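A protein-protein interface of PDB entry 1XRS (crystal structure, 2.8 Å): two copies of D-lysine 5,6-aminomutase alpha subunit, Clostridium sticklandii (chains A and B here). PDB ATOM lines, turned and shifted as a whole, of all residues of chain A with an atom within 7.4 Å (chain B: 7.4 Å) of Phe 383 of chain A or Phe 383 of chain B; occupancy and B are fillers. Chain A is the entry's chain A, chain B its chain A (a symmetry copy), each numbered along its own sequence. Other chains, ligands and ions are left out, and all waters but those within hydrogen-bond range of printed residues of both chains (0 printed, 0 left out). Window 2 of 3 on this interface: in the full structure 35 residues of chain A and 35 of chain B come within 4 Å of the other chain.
Among the printed residues, pairs that only touch across the chains: Phe 383 of chain A with Phe 383 of chain B (3.3 Å), Phe 383 of chain A with Leu 423 of chain B (3.4 Å), Lys 384 of chain A with Glu 426 of chain B (3.8 Å), His 386 of chain A with Ile 387 of chain B (3.7 Å), Ile 387 of chain A with His 386 of chain B (3.7 Å), Leu 423 of chain A with Phe 383 of chain B (3.4 Å) and Glu 426 of chain A with Lys 384 of chain B (3.8 Å).
Phe 383 of chain B touches its own counterpart, Phe 383 of chain A. Phe 383 of chain A touches His 386 of chain B, and with the chains exchanged His 386 of chain A touches Phe 383 of chain B. Phe 383 of chain A touches Leu 423 of chain B, and with the chains exchanged Leu 423 of chain A touches Phe 383 of chain B. His 386 of chain A touches Ile 387 of chain B, and with the chains exchanged Ile 387 of chain A touches His 386 of chain B. 16 positions are printed for both chains. Of the 11 pairs that touch across the chains among the printed residues, 11 have their exchanged pair printed and touching as well.
OG1 of Thr 379 of chain A lies close to N of Asn 381 of chain A. N of Phe 383 of chain A sits close to OD1 of Asn 381 of chain A (3.1 Å). A ring nitrogen (NE2) of His 386 of chain A lies within hydrogen-bond range of the backbone carbonyl oxygen of Leu 423 of chain A, at 3.5 Å. The side-chain amide oxygen (OD1) of Asn 381 of chain B sits close to the backbone NH (N) of Phe 383 of chain B (3.1 Å). The side-chain amide oxygen (OD1) of Asn 381 of chain B lies within hydrogen-bond range of the backbone NH (N) of Lys 384 of chain B. A ring nitrogen (NE2) of His 386 of chain B lies within hydrogen-bond range of the backbone carbonyl oxygen (O) of Leu 423 of chain B, at 3.5 Å.
Of chain B, only Phe 383 (3.3 Å), His 386 (3.4 Å) and Leu 423 (3.4 Å) come within 4 Å of Phe 383 of chain A. Asp 389 of chain A touches none of the printed residues of chain B. Of the printed residues of chain A, Asn 381 of chain B touches Glu 426. Phe 383 of chain B touches three residues of chain A. Printed residues of chain A within 4 Å of His 386 of chain B: Phe 383 and Ile 387. Printed residues of chain A within 4 Å of Leu 423 of chain B: Phe 383. Of the printed residues of chain A, Glu 426 of chain B touches Asn 381 and Lys 384. The nearest residue of chain B that does not touch Phe 383 of chain A is Ile 382 of chain B (4.2 Å). The nearest residue of chain A that does not touch Phe 383 of chain B is Ile 382 of chain A (4.2 Å). The nearest printed residue of chain A that does not touch Lys 384 of chain B is His 386 of chain A (4.6 Å).
Hydrophobic or aromatic side chains of chain A that line the printed part of chain B: Phe 383, His 386, Ile 387 and Leu 423. Printed residues of chain B that touch a printed residue of chain A: Asn 381, Phe 383, Lys 384, His 386, Ile 387, Leu 423 and Glu 426. Hydrophobic or aromatic side chains of chain B that line the printed part of chain A: Phe 383, His 386, Ile 387 and Leu 423. Along chain B the printed residues that touch a printed residue of chain A span positions 381 to 426.
The side-chain carboxylate (OE1) of Glu 426 of chain B sits at hydrogen-bond distance from the side-chain amide nitrogen (ND2) of Asn 381 of chain A (2.8 Å). The backbone carbonyl oxygen of Phe 383 of chain A lies within hydrogen-bond range of a ring nitrogen (ND1) of His 386 of chain B. The backbone carbonyl oxygen (O) of Phe 383 of chain B is in hydrogen-bond range of a ring nitrogen (ND1) of His 386 of chain A (3.4 Å). OE1 of Glu 426 of chain A lies within hydrogen-bond range of ND2 of Asn 381 of chain B.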
ATOM      1  N   THR A 379      23.387  -9.184  11.523  1.00  0.00           N
ATOM      2  CA  THR A 379      24.086  -7.917  11.876  1.00  0.00           C
ATOM      3  C   THR A 379      24.840  -7.253  10.735  1.00  0.00           C
ATOM      4  O   THR A 379      24.655  -7.591   9.566  1.00  0.00           O
ATOM      5  CB  THR A 379      25.134  -8.081  13.014  1.00  0.00           C
ATOM      6  OG1 THR A 379      26.188  -8.951  12.580  1.00  0.00           O
ATOM      7  CG2 THR A 379      24.501  -8.649  14.257  1.00  0.00           C
ATOM      8  N   GLY A 380      25.709  -6.312  11.107  1.00  0.00           N
ATOM      9  CA  GLY A 380      26.498  -5.559  10.141  1.00  0.00           C
ATOM     10  C   GLY A 380      27.614  -6.374   9.537  1.00  0.00           C
ATOM     11  O   GLY A 380      28.266  -5.945   8.567  1.00  0.00           O
ATOM     12  N   ASN A 381      27.823  -7.561  10.113  1.00  0.00           N
ATOM     13  CA  ASN A 381      28.854  -8.479   9.646  1.00  0.00           C
ATOM     14  C   ASN A 381      28.374  -9.207   8.405  1.00  0.00           C
ATOM     15  O   ASN A 381      28.088 -10.391   8.445  1.00  0.00           O
ATOM     16  CB  ASN A 381      29.170  -9.504  10.722  1.00  0.00           C
ATOM     17  CG  ASN A 381      30.362 -10.362  10.358  1.00  0.00           C
ATOM     18  OD1 ASN A 381      30.629 -10.617   9.166  1.00  0.00           O
ATOM     19  ND2 ASN A 381      31.086 -10.825  11.380  1.00  0.00           N
ATOM     20  N   ILE A 382      28.291  -8.502   7.295  1.00  0.00           N
ATOM     21  CA  ILE A 382      27.809  -9.095   6.067  1.00  0.00           C
ATOM     22  C   ILE A 382      28.351 -10.522   5.754  1.00  0.00           C
ATOM     23  O   ILE A 382      27.693 -11.326   5.079  1.00  0.00           O
ATOM     24  CB  ILE A 382      28.112  -8.139   4.914  1.00  0.00           C
ATOM     25  CG1 ILE A 382      27.512  -8.671   3.625  1.00  0.00           C
ATOM     26  CG2 ILE A 382      29.610  -7.960   4.765  1.00  0.00           C
ATOM     27  CD1 ILE A 382      28.081  -8.001   2.401  1.00  0.00           C
ATOM     28  N   PHE A 383      29.538 -10.851   6.252  1.00  0.00           N
ATOM     29  CA  PHE A 383      30.107 -12.165   5.980  1.00  0.00           C
ATOM     30  C   PHE A 383      29.457 -13.300   6.762  1.00  0.00           C
ATOM     31  O   PHE A 383      29.148 -14.362   6.218  1.00  0.00           O
ATOM     32  CB  PHE A 383      31.586 -12.091   6.247  1.00  0.00           C
ATOM     33  CG  PHE A 383      32.237 -11.028   5.470  1.00  0.00           C
ATOM     34  CD1 PHE A 383      32.103 -11.004   4.087  1.00  0.00           C
ATOM     35  CD2 PHE A 383      32.982 -10.045   6.096  1.00  0.00           C
ATOM     36  CE1 PHE A 383      32.706 -10.017   3.320  1.00  0.00           C
ATOM     37  CE2 PHE A 383      33.602  -9.040   5.336  1.00  0.00           C
ATOM     38  CZ  PHE A 383      33.460  -9.031   3.939  1.00  0.00           C
ATOM     39  N   LYS A 384      29.252 -13.051   8.044  1.00  0.00           N
ATOM     40  CA  LYS A 384      28.592 -13.992   8.922  1.00  0.00           C
ATOM     41  C   LYS A 384      27.120 -14.148   8.407  1.00  0.00           C
ATOM     42  O   LYS A 384      26.590 -15.266   8.257  1.00  0.00           O
ATOM     43  CB  LYS A 384      28.654 -13.428  10.355  1.00  0.00           C
ATOM     44  CG  LYS A 384      27.637 -13.983  11.325  1.00  0.00           C
ATOM     45  CD  LYS A 384      27.930 -15.410  11.705  1.00  0.00           C
ATOM     46  CE  LYS A 384      28.361 -15.524  13.175  1.00  0.00           C
ATOM     47  NZ  LYS A 384      27.221 -15.408  14.106  1.00  0.00           N
ATOM     48  N   GLY A 385      26.494 -13.022   8.095  1.00  0.00           N
ATOM     49  CA  GLY A 385      25.135 -13.036   7.619  1.00  0.00           C
ATOM     50  C   GLY A 385      24.918 -13.860   6.378  1.00  0.00           C
ATOM     51  O   GLY A 385      23.883 -14.504   6.229  1.00  0.00           O
ATOM     52  N   HIS A 386      25.878 -13.847   5.471  1.00  0.00           N
ATOM     53  CA  HIS A 386      25.721 -14.626   4.255  1.00  0.00           C
ATOM     54  C   HIS A 386      25.711 -16.116   4.631  1.00  0.00           C
ATOM     55  O   HIS A 386      24.951 -16.899   4.048  1.00  0.00           O
ATOM     56  CB  HIS A 386      26.871 -14.327   3.307  1.00  0.00           C
ATOM     57  CG  HIS A 386      26.561 -14.568   1.864  1.00  0.00           C
ATOM     58  ND1 HIS A 386      27.520 -14.977   0.958  1.00  0.00           N
ATOM     59  CD2 HIS A 386      25.431 -14.373   1.146  1.00  0.00           C
ATOM     60  CE1 HIS A 386      26.995 -15.018  -0.255  1.00  0.00           C
ATOM     61  NE2 HIS A 386      25.728 -14.658  -0.170  1.00  0.00           N
ATOM     62  N   ILE A 387      26.526 -16.510   5.615  1.00  0.00           N
ATOM     63  CA  ILE A 387      26.568 -17.919   5.982  1.00  0.00           C
ATOM     64  C   ILE A 387      25.348 -18.345   6.779  1.00  0.00           C
ATOM     65  O   ILE A 387      24.903 -19.490   6.669  1.00  0.00           O
ATOM     66  CB  ILE A 387      27.906 -18.342   6.731  1.00  0.00           C
ATOM     67  CG1 ILE A 387      27.608 -18.767   8.159  1.00  0.00           C
ATOM     68  CG2 ILE A 387      28.932 -17.250   6.701  1.00  0.00           C
ATOM     69  CD1 ILE A 387      27.163 -20.210   8.261  1.00  0.00           C
ATOM     70  N   GLN A 388      24.780 -17.459   7.589  1.00  0.00           N
ATOM     71  CA  GLN A 388      23.576 -17.885   8.294  1.00  0.00           C
ATOM     72  C   GLN A 388      22.393 -17.881   7.326  1.00  0.00           C
ATOM     73  O   GLN A 388      21.373 -18.474   7.597  1.00  0.00           O
ATOM     74  CB  GLN A 388      23.311 -17.064   9.561  1.00  0.00           C
ATOM     75  CG  GLN A 388      23.393 -15.596   9.425  1.00  0.00           C
ATOM     76  CD  GLN A 388      23.536 -14.907  10.780  1.00  0.00           C
ATOM     77  OE1 GLN A 388      22.817 -15.220  11.742  1.00  0.00           O
ATOM     78  NE2 GLN A 388      24.465 -13.956  10.857  1.00  0.00           N
ATOM     79  N   ASP A 389      22.541 -17.246   6.175  1.00  0.00           N
ATOM     80  CA  ASP A 389      21.486 -17.273   5.168  1.00  0.00           C
ATOM     81  C   ASP A 389      21.664 -18.639   4.490  1.00  0.00           C
ATOM     82  O   ASP A 389      20.728 -19.258   3.987  1.00  0.00           O
ATOM     83  CB  ASP A 389      21.693 -16.144   4.150  1.00  0.00           C
ATOM     84  CG  ASP A 389      20.971 -14.850   4.539  1.00  0.00           C
ATOM     85  OD1 ASP A 389      21.272 -13.782   3.966  1.00  0.00           O
ATOM     86  OD2 ASP A 389      20.087 -14.895   5.421  1.00  0.00           O
ATOM     87  N   LEU A 409      22.334 -10.783   2.672  1.00  0.00           N
ATOM     88  CA  LEU A 409      23.495 -10.571   3.534  1.00  0.00           C
ATOM     89  C   LEU A 409      23.410  -9.191   4.149  1.00  0.00           C
ATOM     90  O   LEU A 409      23.901  -8.966   5.258  1.00  0.00           O
ATOM     91  CB  LEU A 409      24.831 -10.708   2.777  1.00  0.00           C
ATOM     92  CG  LEU A 409      25.168  -9.919   1.511  1.00  0.00           C
ATOM     93  CD1 LEU A 409      26.513 -10.382   0.983  1.00  0.00           C
ATOM     94  CD2 LEU A 409      24.107 -10.176   0.448  1.00  0.00           C
ATOM     95  N   SER A 419      23.456  -6.141  -6.376  1.00  0.00           N
ATOM     96  CA  SER A 419      24.444  -7.104  -5.916  1.00  0.00           C
ATOM     97  C   SER A 419      23.930  -7.975  -4.760  1.00  0.00           C
ATOM     98  O   SER A 419      24.039  -9.210  -4.796  1.00  0.00           O
ATOM     99  CB  SER A 419      25.728  -6.368  -5.519  1.00  0.00           C
ATOM    100  OG  SER A 419      25.713  -5.981  -4.160  1.00  0.00           O
ATOM    101  N   LEU A 423      23.916 -12.168  -5.077  1.00  0.00           N
ATOM    102  CA  LEU A 423      24.668 -12.975  -4.137  1.00  0.00           C
ATOM    103  C   LEU A 423      23.748 -13.917  -3.407  1.00  0.00           C
ATOM    104  O   LEU A 423      24.081 -15.087  -3.206  1.00  0.00           O
ATOM    105  CB  LEU A 423      25.342 -12.073  -3.114  1.00  0.00           C
ATOM    106  CG  LEU A 423      26.534 -11.228  -3.579  1.00  0.00           C
ATOM    107  CD1 LEU A 423      27.093 -10.474  -2.386  1.00  0.00           C
ATOM    108  CD2 LEU A 423      27.618 -12.140  -4.175  1.00  0.00           C
ATOM    109  N   GLU A 426      22.648 -16.667  -5.800  1.00  0.00           N
ATOM    110  CA  GLU A 426      23.657 -17.675  -6.113  1.00  0.00           C
ATOM    111  C   GLU A 426      23.883 -18.571  -4.890  1.00  0.00           C
ATOM    112  O   GLU A 426      24.053 -19.793  -5.028  1.00  0.00           O
ATOM    113  CB  GLU A 426      24.974 -17.037  -6.609  1.00  0.00           C
ATOM    114  CG  GLU A 426      25.876 -16.396  -5.564  1.00  0.00           C
ATOM    115  CD  GLU A 426      27.263 -16.009  -6.124  1.00  0.00           C
ATOM    116  OE1 GLU A 426      28.036 -15.319  -5.422  1.00  0.00           O
ATOM    117  OE2 GLU A 426      27.583 -16.397  -7.264  1.00  0.00           O
ATOM    118  N   ASN A 427      23.830 -17.963  -3.701  1.00  0.00           N
ATOM    119  CA  ASN A 427      24.018 -18.701  -2.460  1.00  0.00           C
ATOM    120  C   ASN A 427      22.938 -19.787  -2.406  1.00  0.00           C
ATOM    121  O   ASN A 427      23.220 -20.966  -2.161  1.00  0.00           O
ATOM    122  CB  ASN A 427      23.892 -17.754  -1.256  1.00  0.00           C
ATOM    123  CG  ASN A 427      24.028 -18.483   0.093  1.00  0.00           C
ATOM    124  OD1 ASN A 427      23.812 -19.693   0.166  1.00  0.00           O
ATOM    125  ND2 ASN A 427      24.358 -17.739   1.169  1.00  0.00           N
ATOM    126  N   THR B 379      37.274 -18.803  -6.008  1.00  0.00           N
ATOM    127  CA  THR B 379      37.545 -17.656  -6.917  1.00  0.00           C
ATOM    128  C   THR B 379      37.604 -16.294  -6.243  1.00  0.00           C
ATOM    129  O   THR B 379      37.695 -16.191  -5.021  1.00  0.00           O
ATOM    130  CB  THR B 379      36.492 -17.501  -8.054  1.00  0.00           C
ATOM    131  OG1 THR B 379      35.210 -17.202  -7.488  1.00  0.00           O
ATOM    132  CG2 THR B 379      36.393 -18.759  -8.876  1.00  0.00           C
ATOM    133  N   GLY B 380      37.532 -15.252  -7.074  1.00  0.00           N
ATOM    134  CA  GLY B 380      37.598 -13.876  -6.599  1.00  0.00           C
ATOM    135  C   GLY B 380      36.330 -13.436  -5.908  1.00  0.00           C
ATOM    136  O   GLY B 380      36.282 -12.359  -5.285  1.00  0.00           O
ATOM    137  N   ASN B 381      35.304 -14.285  -6.015  1.00  0.00           N
ATOM    138  CA  ASN B 381      34.011 -14.020  -5.397  1.00  0.00           C
ATOM    139  C   ASN B 381      34.072 -14.336  -3.915  1.00  0.00           C
ATOM    140  O   ASN B 381      33.492 -15.307  -3.458  1.00  0.00           O
ATOM    141  CB  ASN B 381      32.938 -14.882  -6.038  1.00  0.00           C
ATOM    142  CG  ASN B 381      31.550 -14.511  -5.561  1.00  0.00           C
ATOM    143  OD1 ASN B 381      31.366 -14.047  -4.417  1.00  0.00           O
ATOM    144  ND2 ASN B 381      30.556 -14.719  -6.428  1.00  0.00           N
ATOM    145  N   ILE B 382      34.768 -13.514  -3.157  1.00  0.00           N
ATOM    146  CA  ILE B 382      34.917 -13.749  -1.738  1.00  0.00           C
ATOM    147  C   ILE B 382      33.623 -14.195  -0.993  1.00  0.00           C
ATOM    148  O   ILE B 382      33.679 -14.894   0.029  1.00  0.00           O
ATOM    149  CB  ILE B 382      35.503 -12.492  -1.095  1.00  0.00           C
ATOM    150  CG1 ILE B 382      35.789 -12.743   0.374  1.00  0.00           C
ATOM    151  CG2 ILE B 382      34.543 -11.330  -1.256  1.00  0.00           C
ATOM    152  CD1 ILE B 382      36.000 -11.469   1.150  1.00  0.00           C
ATOM    153  N   PHE B 383      32.459 -13.813  -1.503  1.00  0.00           N
ATOM    154  CA  PHE B 383      31.212 -14.183  -0.843  1.00  0.00           C
ATOM    155  C   PHE B 383      30.821 -15.644  -1.027  1.00  0.00           C
ATOM    156  O   PHE B 383      30.428 -16.328  -0.079  1.00  0.00           O
ATOM    157  CB  PHE B 383      30.135 -13.258  -1.340  1.00  0.00           C
ATOM    158  CG  PHE B 383      30.477 -11.845  -1.135  1.00  0.00           C
ATOM    159  CD1 PHE B 383      30.803 -11.393   0.138  1.00  0.00           C
ATOM    160  CD2 PHE B 383      30.485 -10.955  -2.193  1.00  0.00           C
ATOM    161  CE1 PHE B 383      31.130 -10.064   0.372  1.00  0.00           C
ATOM    162  CE2 PHE B 383      30.810  -9.606  -1.975  1.00  0.00           C
ATOM    163  CZ  PHE B 383      31.133  -9.163  -0.683  1.00  0.00           C
ATOM    164  N   LYS B 384      30.940 -16.106  -2.259  1.00  0.00           N
ATOM    165  CA  LYS B 384      30.668 -17.484  -2.602  1.00  0.00           C
ATOM    166  C   LYS B 384      31.725 -18.363  -1.848  1.00  0.00           C
ATOM    167  O   LYS B 384      31.399 -19.379  -1.206  1.00  0.00           O
ATOM    168  CB  LYS B 384      30.778 -17.622  -4.133  1.00  0.00           C
ATOM    169  CG  LYS B 384      31.010 -19.022  -4.653  1.00  0.00           C
ATOM    170  CD  LYS B 384      29.794 -19.896  -4.501  1.00  0.00           C
ATOM    171  CE  LYS B 384      29.178 -20.244  -5.866  1.00  0.00           C
ATOM    172  NZ  LYS B 384      29.948 -21.276  -6.585  1.00  0.00           N
ATOM    173  N   GLY B 385      32.977 -17.929  -1.896  1.00  0.00           N
ATOM    174  CA  GLY B 385      34.040 -18.656  -1.249  1.00  0.00           C
ATOM    175  C   GLY B 385      33.843 -18.862   0.229  1.00  0.00           C
ATOM    176  O   GLY B 385      34.200 -19.906   0.768  1.00  0.00           O
ATOM    177  N   HIS B 386      33.284 -17.874   0.905  1.00  0.00           N
ATOM    178  CA  HIS B 386      33.071 -18.020   2.335  1.00  0.00           C
ATOM    179  C   HIS B 386      32.035 -19.133   2.560  1.00  0.00           C
ATOM    180  O   HIS B 386      32.165 -19.921   3.504  1.00  0.00           O
ATOM    181  CB  HIS B 386      32.568 -16.707   2.911  1.00  0.00           C
ATOM    182  CG  HIS B 386      32.856 -16.519   4.366  1.00  0.00           C
ATOM    183  ND1 HIS B 386      32.019 -15.805   5.202  1.00  0.00           N
ATOM    184  CD2 HIS B 386      33.924 -16.867   5.119  1.00  0.00           C
ATOM    185  CE1 HIS B 386      32.563 -15.717   6.404  1.00  0.00           C
ATOM    186  NE2 HIS B 386      33.719 -16.355   6.383  1.00  0.00           N
ATOM    187  N   ILE B 387      31.025 -19.222   1.687  1.00  0.00           N
ATOM    188  CA  ILE B 387      30.007 -20.246   1.881  1.00  0.00           C
ATOM    189  C   ILE B 387      30.500 -21.631   1.501  1.00  0.00           C
ATOM    190  O   ILE B 387      30.086 -22.624   2.105  1.00  0.00           O
ATOM    191  CB  ILE B 387      28.630 -19.919   1.154  1.00  0.00           C
ATOM    192  CG1 ILE B 387      28.351 -20.934   0.059  1.00  0.00           C
ATOM    193  CG2 ILE B 387      28.603 -18.523   0.610  1.00  0.00           C
ATOM    194  CD1 ILE B 387      27.708 -22.200   0.581  1.00  0.00           C
ATOM    195  N   GLN B 388      31.380 -21.741   0.513  1.00  0.00           N
ATOM    196  CA  GLN B 388      31.874 -23.081   0.216  1.00  0.00           C
ATOM    197  C   GLN B 388      32.893 -23.493   1.277  1.00  0.00           C
ATOM    198  O   GLN B 388      33.210 -24.653   1.411  1.00  0.00           O
ATOM    199  CB  GLN B 388      32.419 -23.205  -1.213  1.00  0.00           C
ATOM    200  CG  GLN B 388      33.350 -22.150  -1.659  1.00  0.00           C
ATOM    201  CD  GLN B 388      33.494 -22.125  -3.178  1.00  0.00           C
ATOM    202  OE1 GLN B 388      33.668 -23.168  -3.827  1.00  0.00           O
ATOM    203  NE2 GLN B 388      33.428 -20.925  -3.751  1.00  0.00           N
ATOM    204  N   ASP B 389      33.381 -22.546   2.063  1.00  0.00           N
ATOM    205  CA  ASP B 389      34.292 -22.879   3.153  1.00  0.00           C
ATOM    206  C   ASP B 389      33.360 -23.387   4.264  1.00  0.00           C
ATOM    207  O   ASP B 389      33.716 -24.215   5.101  1.00  0.00           O
ATOM    208  CB  ASP B 389      35.042 -21.625   3.621  1.00  0.00           C
ATOM    209  CG  ASP B 389      36.368 -21.413   2.885  1.00  0.00           C
ATOM    210  OD1 ASP B 389      36.941 -20.305   2.956  1.00  0.00           O
ATOM    211  OD2 ASP B 389      36.854 -22.361   2.232  1.00  0.00           O
ATOM    212  N   LEU B 409      38.340 -17.172   2.835  1.00  0.00           N
ATOM    213  CA  LEU B 409      37.496 -16.594   1.792  1.00  0.00           C
ATOM    214  C   LEU B 409      38.377 -15.992   0.719  1.00  0.00           C
ATOM    215  O   LEU B 409      37.996 -15.943  -0.453  1.00  0.00           O
ATOM    216  CB  LEU B 409      36.540 -15.513   2.331  1.00  0.00           C
ATOM    217  CG  LEU B 409      37.007 -14.298   3.135  1.00  0.00           C
ATOM    218  CD1 LEU B 409      35.793 -13.507   3.588  1.00  0.00           C
ATOM    219  CD2 LEU B 409      37.779 -14.762   4.364  1.00  0.00           C
ATOM    220  N   SER B 419      41.966  -9.990   9.156  1.00  0.00           N
ATOM    221  CA  SER B 419      40.534 -10.134   8.952  1.00  0.00           C
ATOM    222  C   SER B 419      40.158 -11.477   8.307  1.00  0.00           C
ATOM    223  O   SER B 419      39.268 -12.190   8.792  1.00  0.00           O
ATOM    224  CB  SER B 419      40.016  -8.960   8.114  1.00  0.00           C
ATOM    225  OG  SER B 419      40.076  -9.236   6.730  1.00  0.00           O
ATOM    226  N   LEU B 423      37.445 -14.079  10.190  1.00  0.00           N
ATOM    227  CA  LEU B 423      36.214 -14.460   9.525  1.00  0.00           C
ATOM    228  C   LEU B 423      36.157 -15.955   9.357  1.00  0.00           C
ATOM    229  O   LEU B 423      35.107 -16.568   9.567  1.00  0.00           O
ATOM    230  CB  LEU B 423      36.160 -13.818   8.146  1.00  0.00           C
ATOM    231  CG  LEU B 423      35.914 -12.307   8.068  1.00  0.00           C
ATOM    232  CD1 LEU B 423      35.821 -11.904   6.608  1.00  0.00           C
ATOM    233  CD2 LEU B 423      34.606 -11.955   8.793  1.00  0.00           C
ATOM    234  N   GLU B 426      35.510 -17.552  12.753  1.00  0.00           N
ATOM    235  CA  GLU B 426      34.152 -17.418  13.268  1.00  0.00           C
ATOM    236  C   GLU B 426      33.206 -18.313  12.457  1.00  0.00           C
ATOM    237  O   GLU B 426      32.294 -18.939  13.022  1.00  0.00           O
ATOM    238  CB  GLU B 426      33.682 -15.946  13.277  1.00  0.00           C
ATOM    239  CG  GLU B 426      33.283 -15.332  11.942  1.00  0.00           C
ATOM    240  CD  GLU B 426      32.607 -13.952  12.094  1.00  0.00           C
ATOM    241  OE1 GLU B 426      32.387 -13.261  11.074  1.00  0.00           O
ATOM    242  OE2 GLU B 426      32.288 -13.558  13.234  1.00  0.00           O
ATOM    243  N   ASN B 427      33.466 -18.407  11.150  1.00  0.00           N
ATOM    244  CA  ASN B 427      32.652 -19.231  10.269  1.00  0.00           C
ATOM    245  C   ASN B 427      32.718 -20.667  10.797  1.00  0.00           C
ATOM    246  O   ASN B 427      31.693 -21.337  10.978  1.00  0.00           O
ATOM    247  CB  ASN B 427      33.186 -19.160   8.830  1.00  0.00           C
ATOM    248  CG  ASN B 427      32.398 -20.052   7.855  1.00  0.00           C
ATOM    249  OD1 ASN B 427      31.746 -21.006   8.282  1.00  0.00           O
ATOM    250  ND2 ASN B 427      32.483 -19.762   6.540  1.00  0.00           N
